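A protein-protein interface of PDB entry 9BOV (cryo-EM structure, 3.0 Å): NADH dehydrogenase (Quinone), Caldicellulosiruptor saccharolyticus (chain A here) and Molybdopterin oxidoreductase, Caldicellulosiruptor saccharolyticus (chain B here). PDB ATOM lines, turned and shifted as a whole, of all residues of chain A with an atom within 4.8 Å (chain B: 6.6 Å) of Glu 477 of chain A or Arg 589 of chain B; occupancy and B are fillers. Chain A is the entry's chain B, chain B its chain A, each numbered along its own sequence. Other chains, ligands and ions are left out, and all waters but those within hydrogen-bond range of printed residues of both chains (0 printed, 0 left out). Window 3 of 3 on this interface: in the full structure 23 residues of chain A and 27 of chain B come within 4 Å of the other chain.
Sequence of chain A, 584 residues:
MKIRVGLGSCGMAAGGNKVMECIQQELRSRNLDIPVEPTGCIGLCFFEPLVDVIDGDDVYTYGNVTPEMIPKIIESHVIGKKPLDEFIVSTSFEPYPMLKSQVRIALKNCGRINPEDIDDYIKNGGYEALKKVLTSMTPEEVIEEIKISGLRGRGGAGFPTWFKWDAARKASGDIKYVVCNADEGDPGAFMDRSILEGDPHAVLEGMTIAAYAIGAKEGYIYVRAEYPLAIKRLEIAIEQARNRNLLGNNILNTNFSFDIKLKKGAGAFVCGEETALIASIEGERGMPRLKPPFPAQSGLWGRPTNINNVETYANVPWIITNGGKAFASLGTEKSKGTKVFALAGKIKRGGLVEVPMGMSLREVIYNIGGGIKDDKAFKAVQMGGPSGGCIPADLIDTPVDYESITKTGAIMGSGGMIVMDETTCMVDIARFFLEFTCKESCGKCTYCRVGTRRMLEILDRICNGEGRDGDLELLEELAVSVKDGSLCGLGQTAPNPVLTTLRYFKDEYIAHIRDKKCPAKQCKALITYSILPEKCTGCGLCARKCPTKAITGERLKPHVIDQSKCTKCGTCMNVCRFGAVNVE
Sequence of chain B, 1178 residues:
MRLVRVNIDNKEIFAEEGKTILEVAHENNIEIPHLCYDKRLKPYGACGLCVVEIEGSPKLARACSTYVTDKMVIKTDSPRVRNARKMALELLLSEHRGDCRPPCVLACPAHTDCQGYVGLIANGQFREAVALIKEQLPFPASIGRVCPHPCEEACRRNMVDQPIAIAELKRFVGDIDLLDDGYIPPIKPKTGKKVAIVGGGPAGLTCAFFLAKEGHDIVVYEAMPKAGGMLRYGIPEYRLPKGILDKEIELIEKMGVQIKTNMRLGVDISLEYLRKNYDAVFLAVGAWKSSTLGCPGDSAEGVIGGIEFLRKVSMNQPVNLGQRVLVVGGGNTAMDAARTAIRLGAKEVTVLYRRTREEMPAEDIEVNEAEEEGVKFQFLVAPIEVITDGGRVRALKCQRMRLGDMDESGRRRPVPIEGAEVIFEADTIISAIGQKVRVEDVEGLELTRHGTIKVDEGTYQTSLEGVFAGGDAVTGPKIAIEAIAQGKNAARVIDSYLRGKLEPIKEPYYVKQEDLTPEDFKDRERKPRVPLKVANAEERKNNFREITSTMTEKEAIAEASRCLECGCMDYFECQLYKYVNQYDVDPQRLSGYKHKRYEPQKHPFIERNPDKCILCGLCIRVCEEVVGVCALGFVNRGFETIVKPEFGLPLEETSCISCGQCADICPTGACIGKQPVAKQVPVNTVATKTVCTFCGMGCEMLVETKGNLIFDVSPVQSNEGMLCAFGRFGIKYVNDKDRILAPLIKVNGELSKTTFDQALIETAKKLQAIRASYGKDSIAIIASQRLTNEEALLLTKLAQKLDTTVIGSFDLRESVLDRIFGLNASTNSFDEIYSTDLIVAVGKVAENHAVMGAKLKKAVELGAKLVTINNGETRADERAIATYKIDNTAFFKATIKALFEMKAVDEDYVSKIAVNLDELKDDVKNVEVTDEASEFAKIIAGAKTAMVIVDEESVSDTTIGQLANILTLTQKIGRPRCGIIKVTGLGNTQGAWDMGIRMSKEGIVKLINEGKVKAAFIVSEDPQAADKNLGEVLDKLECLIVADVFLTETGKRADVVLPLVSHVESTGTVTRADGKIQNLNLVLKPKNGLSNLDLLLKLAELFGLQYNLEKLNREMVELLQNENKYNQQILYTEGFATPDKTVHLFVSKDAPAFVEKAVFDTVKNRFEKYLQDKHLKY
The side-chain sulfur (SD) of Met 87 of chain B is in hydrogen-bond range of the side-chain hydroxyl (OG) of Ser 481 of chain A (3.5 Å). NH2 of Arg 589 of chain B is in salt-bridge range of OE2 of Glu 477 of chain A (2.5 Å).
The backbone carbonyl oxygen (O) of Glu 477 of chain A is in hydrogen-bond range of the side-chain hydroxyl (OG) of Ser 481 of chain A (2.5 Å). O of Leu 478 of chain A lies within hydrogen-bond range of OG of Ser 481 of chain A, at 2.8 Å.
Among the printed residues, merely in contact across the chains: Leu 474 of chain A with Arg 589 of chain B (3.3 Å), Leu 474 of chain A with Leu 590 of chain B (3.8 Å), Glu 477 of chain A with Met 87 of chain B (3.4 Å), Leu 478 of chain A with Met 87 of chain B (3.9 Å) and Leu 478 of chain A with Leu 590 of chain B (3.6 Å).
Of the printed residues of chain B, Leu 474 of chain A touches Arg 589 (3.3 Å) and Leu 590 (3.8 Å). Leu 475 of chain A touches none of the printed residues of chain B. Glu 476 of chain A touches none of the printed residues of chain B. Glu 477 of chain A touches two residues of chain B. Of the printed residues of chain B, Leu 478 of chain A touches Met 87 (3.9 Å) and Leu 590 (3.6 Å). Printed residues of chain A within 4 Å of Met 87 of chain B: Glu 477 (3.4 Å), Leu 478 (3.9 Å) and Ser 481 (3.5 Å). Arg 589 of chain B touches just these residues of chain A: Leu 474 and Glu 477. Of the printed residues of chain A, Leu 590 of chain B touches Leu 474 and Leu 478. The nearest residue of chain B that does not touch Glu 477 of chain A is Lys 86 of chain B (4.04 Å). The nearest printed residue of chain B that does not touch Leu 474 of chain A is Met 87 of chain B (6.2 Å).
Hydrophobic or aromatic side chains of chain B within 4 Å of the printed part of chain A: Met 87 and Leu 590. Printed residues of chain A that touch a printed residue of chain B: Leu 474, Glu 477, Leu 478 and Ser 481. Hydrophobic or aromatic side chains of chain A that line the printed part of chain B: Leu 474 and Leu 478.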
ATOM      1  N   GLU A 473     -27.160  21.724 -23.242  1.00  0.00           N
ATOM      2  CA  GLU A 473     -25.990  21.238 -23.967  1.00  0.00           C
ATOM      3  C   GLU A 473     -24.708  21.842 -23.408  1.00  0.00           C
ATOM      4  O   GLU A 473     -23.700  21.143 -23.249  1.00  0.00           O
ATOM      5  CB  GLU A 473     -26.132  21.551 -25.456  1.00  0.00           C
ATOM      6  CG  GLU A 473     -27.420  21.034 -26.082  1.00  0.00           C
ATOM      7  CD  GLU A 473     -28.535  22.062 -26.065  1.00  0.00           C
ATOM      8  OE1 GLU A 473     -28.485  22.979 -25.219  1.00  0.00           O
ATOM      9  OE2 GLU A 473     -29.462  21.954 -26.896  1.00  0.00           O
ATOM     10  N   LEU A 474     -24.730  23.142 -23.100  1.00  0.00           N
ATOM     11  CA  LEU A 474     -23.556  23.791 -22.529  1.00  0.00           C
ATOM     12  C   LEU A 474     -23.220  23.208 -21.163  1.00  0.00           C
ATOM     13  O   LEU A 474     -22.049  22.973 -20.855  1.00  0.00           O
ATOM     14  CB  LEU A 474     -23.790  25.299 -22.433  1.00  0.00           C
ATOM     15  CG  LEU A 474     -22.930  26.166 -21.509  1.00  0.00           C
ATOM     16  CD1 LEU A 474     -21.440  25.977 -21.761  1.00  0.00           C
ATOM     17  CD2 LEU A 474     -23.318  27.632 -21.647  1.00  0.00           C
ATOM     18  N   LEU A 475     -24.237  22.962 -20.334  1.00  0.00           N
ATOM     19  CA  LEU A 475     -24.003  22.376 -19.019  1.00  0.00           C
ATOM     20  C   LEU A 475     -23.430  20.972 -19.131  1.00  0.00           C
ATOM     21  O   LEU A 475     -22.498  20.615 -18.402  1.00  0.00           O
ATOM     22  CB  LEU A 475     -25.305  22.360 -18.220  1.00  0.00           C
ATOM     23  CG  LEU A 475     -25.244  21.831 -16.788  1.00  0.00           C
ATOM     24  CD1 LEU A 475     -24.265  22.633 -15.969  1.00  0.00           C
ATOM     25  CD2 LEU A 475     -26.617  21.869 -16.152  1.00  0.00           C
ATOM     26  N   GLU A 476     -23.970  20.158 -20.041  1.00  0.00           N
ATOM     27  CA  GLU A 476     -23.458  18.803 -20.208  1.00  0.00           C
ATOM     28  C   GLU A 476     -22.021  18.815 -20.710  1.00  0.00           C
ATOM     29  O   GLU A 476     -21.177  18.052 -20.219  1.00  0.00           O
ATOM     30  CB  GLU A 476     -24.353  18.018 -21.165  1.00  0.00           C
ATOM     31  CG  GLU A 476     -23.818  16.646 -21.538  1.00  0.00           C
ATOM     32  CD  GLU A 476     -24.198  15.574 -20.534  1.00  0.00           C
ATOM     33  OE1 GLU A 476     -24.302  15.887 -19.331  1.00  0.00           O
ATOM     34  OE2 GLU A 476     -24.395  14.412 -20.949  1.00  0.00           O
ATOM     35  N   GLU A 477     -21.720  19.678 -21.683  1.00  0.00           N
ATOM     36  CA  GLU A 477     -20.357  19.766 -22.198  1.00  0.00           C
ATOM     37  C   GLU A 477     -19.395  20.270 -21.130  1.00  0.00           C
ATOM     38  O   GLU A 477     -18.277  19.758 -21.001  1.00  0.00           O
ATOM     39  CB  GLU A 477     -20.323  20.668 -23.431  1.00  0.00           C
ATOM     40  CG  GLU A 477     -18.931  21.072 -23.872  1.00  0.00           C
ATOM     41  CD  GLU A 477     -18.945  21.921 -25.127  1.00  0.00           C
ATOM     42  OE1 GLU A 477     -19.705  21.589 -26.060  1.00  0.00           O
ATOM     43  OE2 GLU A 477     -18.199  22.920 -25.182  1.00  0.00           O
ATOM     44  N   LEU A 478     -19.820  21.255 -20.337  1.00  0.00           N
ATOM     45  CA  LEU A 478     -18.985  21.744 -19.249  1.00  0.00           C
ATOM     46  C   LEU A 478     -18.722  20.649 -18.228  1.00  0.00           C
ATOM     47  O   LEU A 478     -17.596  20.502 -17.742  1.00  0.00           O
ATOM     48  CB  LEU A 478     -19.646  22.946 -18.582  1.00  0.00           C
ATOM     49  CG  LEU A 478     -18.838  23.615 -17.474  1.00  0.00           C
ATOM     50  CD1 LEU A 478     -17.405  23.837 -17.914  1.00  0.00           C
ATOM     51  CD2 LEU A 478     -19.486  24.918 -17.077  1.00  0.00           C
ATOM     52  N   ALA A 479     -19.748  19.868 -17.891  1.00  0.00           N
ATOM     53  CA  ALA A 479     -19.571  18.805 -16.910  1.00  0.00           C
ATOM     54  C   ALA A 479     -18.629  17.725 -17.423  1.00  0.00           C
ATOM     55  O   ALA A 479     -17.752  17.262 -16.686  1.00  0.00           O
ATOM     56  CB  ALA A 479     -20.924  18.210 -16.537  1.00  0.00           C
ATOM     57  N   VAL A 480     -18.778  17.318 -18.687  1.00  0.00           N
ATOM     58  CA  VAL A 480     -17.911  16.256 -19.186  1.00  0.00           C
ATOM     59  C   VAL A 480     -16.499  16.773 -19.411  1.00  0.00           C
ATOM     60  O   VAL A 480     -15.541  15.993 -19.391  1.00  0.00           O
ATOM     61  CB  VAL A 480     -18.479  15.615 -20.467  1.00  0.00           C
ATOM     62  CG1 VAL A 480     -19.764  14.873 -20.168  1.00  0.00           C
ATOM     63  CG2 VAL A 480     -18.681  16.645 -21.551  1.00  0.00           C
ATOM     64  N   SER A 481     -16.333  18.078 -19.627  1.00  0.00           N
ATOM     65  CA  SER A 481     -14.984  18.609 -19.783  1.00  0.00           C
ATOM     66  C   SER A 481     -14.292  18.794 -18.437  1.00  0.00           C
ATOM     67  O   SER A 481     -13.082  18.577 -18.326  1.00  0.00           O
ATOM     68  CB  SER A 481     -15.024  19.926 -20.551  1.00  0.00           C
ATOM     69  OG  SER A 481     -16.107  20.729 -20.127  1.00  0.00           O
ATOM     70  N   LYS B  86      -9.348  23.965 -25.879  1.00  0.00           N
ATOM     71  CA  LYS B  86     -10.281  25.068 -26.076  1.00  0.00           C
ATOM     72  C   LYS B  86     -11.138  25.293 -24.839  1.00  0.00           C
ATOM     73  O   LYS B  86     -11.382  26.440 -24.446  1.00  0.00           O
ATOM     74  CB  LYS B  86     -11.156  24.796 -27.300  1.00  0.00           C
ATOM     75  CG  LYS B  86     -12.420  25.630 -27.370  1.00  0.00           C
ATOM     76  CD  LYS B  86     -13.292  25.205 -28.536  1.00  0.00           C
ATOM     77  CE  LYS B  86     -14.709  24.901 -28.085  1.00  0.00           C
ATOM     78  NZ  LYS B  86     -14.760  23.752 -27.141  1.00  0.00           N
ATOM     79  N   MET B  87     -11.604  24.215 -24.209  1.00  0.00           N
ATOM     80  CA  MET B  87     -12.380  24.367 -22.983  1.00  0.00           C
ATOM     81  C   MET B  87     -11.531  24.953 -21.863  1.00  0.00           C
ATOM     82  O   MET B  87     -12.005  25.804 -21.101  1.00  0.00           O
ATOM     83  CB  MET B  87     -12.975  23.028 -22.561  1.00  0.00           C
ATOM     84  CG  MET B  87     -13.649  23.063 -21.203  1.00  0.00           C
ATOM     85  SD  MET B  87     -15.234  23.922 -21.212  1.00  0.00           S
ATOM     86  CE  MET B  87     -15.994  23.233 -22.679  1.00  0.00           C
ATOM     87  N   GLU B  90     -11.198  28.654 -22.586  1.00  0.00           N
ATOM     88  CA  GLU B  90     -12.444  29.354 -22.288  1.00  0.00           C
ATOM     89  C   GLU B  90     -12.630  29.526 -20.787  1.00  0.00           C
ATOM     90  O   GLU B  90     -13.052  30.592 -20.321  1.00  0.00           O
ATOM     91  CB  GLU B  90     -13.629  28.597 -22.885  1.00  0.00           C
ATOM     92  CG  GLU B  90     -13.783  28.753 -24.384  1.00  0.00           C
ATOM     93  CD  GLU B  90     -14.939  27.941 -24.935  1.00  0.00           C
ATOM     94  OE1 GLU B  90     -15.402  27.015 -24.235  1.00  0.00           O
ATOM     95  OE2 GLU B  90     -15.384  28.224 -26.065  1.00  0.00           O
ATOM     96  N   ASP B 586     -14.934  30.306 -27.567  1.00  0.00           N
ATOM     97  CA  ASP B 586     -16.123  31.133 -27.393  1.00  0.00           C
ATOM     98  C   ASP B 586     -16.258  31.469 -25.916  1.00  0.00           C
ATOM     99  O   ASP B 586     -16.692  30.618 -25.124  1.00  0.00           O
ATOM    100  CB  ASP B 586     -17.372  30.407 -27.900  1.00  0.00           C
ATOM    101  CG  ASP B 586     -18.612  31.278 -27.852  1.00  0.00           C
ATOM    102  OD1 ASP B 586     -18.498  32.491 -28.118  1.00  0.00           O
ATOM    103  OD2 ASP B 586     -19.701  30.746 -27.556  1.00  0.00           O
ATOM    104  N   PRO B 587     -15.890  32.678 -25.487  1.00  0.00           N
ATOM    105  CA  PRO B 587     -15.897  32.981 -24.051  1.00  0.00           C
ATOM    106  C   PRO B 587     -17.257  33.367 -23.499  1.00  0.00           C
ATOM    107  O   PRO B 587     -17.452  33.282 -22.279  1.00  0.00           O
ATOM    108  CB  PRO B 587     -14.918  34.152 -23.945  1.00  0.00           C
ATOM    109  CG  PRO B 587     -15.090  34.862 -25.249  1.00  0.00           C
ATOM    110  CD  PRO B 587     -15.368  33.801 -26.285  1.00  0.00           C
ATOM    111  N   GLN B 588     -18.195  33.792 -24.348  1.00  0.00           N
ATOM    112  CA  GLN B 588     -19.463  34.322 -23.855  1.00  0.00           C
ATOM    113  C   GLN B 588     -20.290  33.251 -23.156  1.00  0.00           C
ATOM    114  O   GLN B 588     -20.967  33.534 -22.161  1.00  0.00           O
ATOM    115  CB  GLN B 588     -20.251  34.942 -25.007  1.00  0.00           C
ATOM    116  CG  GLN B 588     -21.558  35.590 -24.588  1.00  0.00           C
ATOM    117  CD  GLN B 588     -22.113  36.518 -25.648  1.00  0.00           C
ATOM    118  OE1 GLN B 588     -21.364  37.121 -26.416  1.00  0.00           O
ATOM    119  NE2 GLN B 588     -23.435  36.639 -25.695  1.00  0.00           N
ATOM    120  N   ARG B 589     -20.253  32.015 -23.663  1.00  0.00           N
ATOM    121  CA  ARG B 589     -21.074  30.952 -23.090  1.00  0.00           C
ATOM    122  C   ARG B 589     -20.711  30.674 -21.638  1.00  0.00           C
ATOM    123  O   ARG B 589     -21.597  30.420 -20.815  1.00  0.00           O
ATOM    124  CB  ARG B 589     -20.930  29.679 -23.921  1.00  0.00           C
ATOM    125  CG  ARG B 589     -19.576  29.538 -24.580  1.00  0.00           C
ATOM    126  CD  ARG B 589     -19.452  28.243 -25.360  1.00  0.00           C
ATOM    127  NE  ARG B 589     -19.514  27.070 -24.498  1.00  0.00           N
ATOM    128  CZ  ARG B 589     -19.254  25.834 -24.902  1.00  0.00           C
ATOM    129  NH1 ARG B 589     -18.914  25.573 -26.154  1.00  0.00           N
ATOM    130  NH2 ARG B 589     -19.335  24.836 -24.028  1.00  0.00           N
ATOM    131  N   LEU B 590     -19.424  30.716 -21.304  1.00  0.00           N
ATOM    132  CA  LEU B 590     -18.955  30.416 -19.960  1.00  0.00           C
ATOM    133  C   LEU B 590     -18.763  31.664 -19.109  1.00  0.00           C
ATOM    134  O   LEU B 590     -18.303  31.555 -17.970  1.00  0.00           O
ATOM    135  CB  LEU B 590     -17.647  29.625 -20.026  1.00  0.00           C
ATOM    136  CG  LEU B 590     -17.794  28.186 -20.517  1.00  0.00           C
ATOM    137  CD1 LEU B 590     -16.440  27.522 -20.666  1.00  0.00           C
ATOM    138  CD2 LEU B 590     -18.682  27.397 -19.576  1.00  0.00           C
ATOM    139  N   SER B 591     -19.096  32.841 -19.630  1.00  0.00           N
ATOM    140  CA  SER B 591     -18.910  34.070 -18.871  1.00  0.00           C
ATOM    141  C   SER B 591     -19.830  34.097 -17.658  1.00  0.00           C
ATOM    142  O   SER B 591     -20.999  33.708 -17.733  1.00  0.00           O
ATOM    143  CB  SER B 591     -19.171  35.287 -19.756  1.00  0.00           C
ATOM    144  OG  SER B 591     -20.528  35.689 -19.684  1.00  0.00           O
ATOM    145  N   GLY B 592     -19.295  34.564 -16.534  1.00  0.00           N
ATOM    146  CA  GLY B 592     -20.052  34.632 -15.301  1.00  0.00           C
ATOM    147  C   GLY B 592     -19.442  35.592 -14.301  1.00  0.00           C
ATOM    148  O   GLY B 592     -18.990  36.677 -14.675  1.00  0.00           O
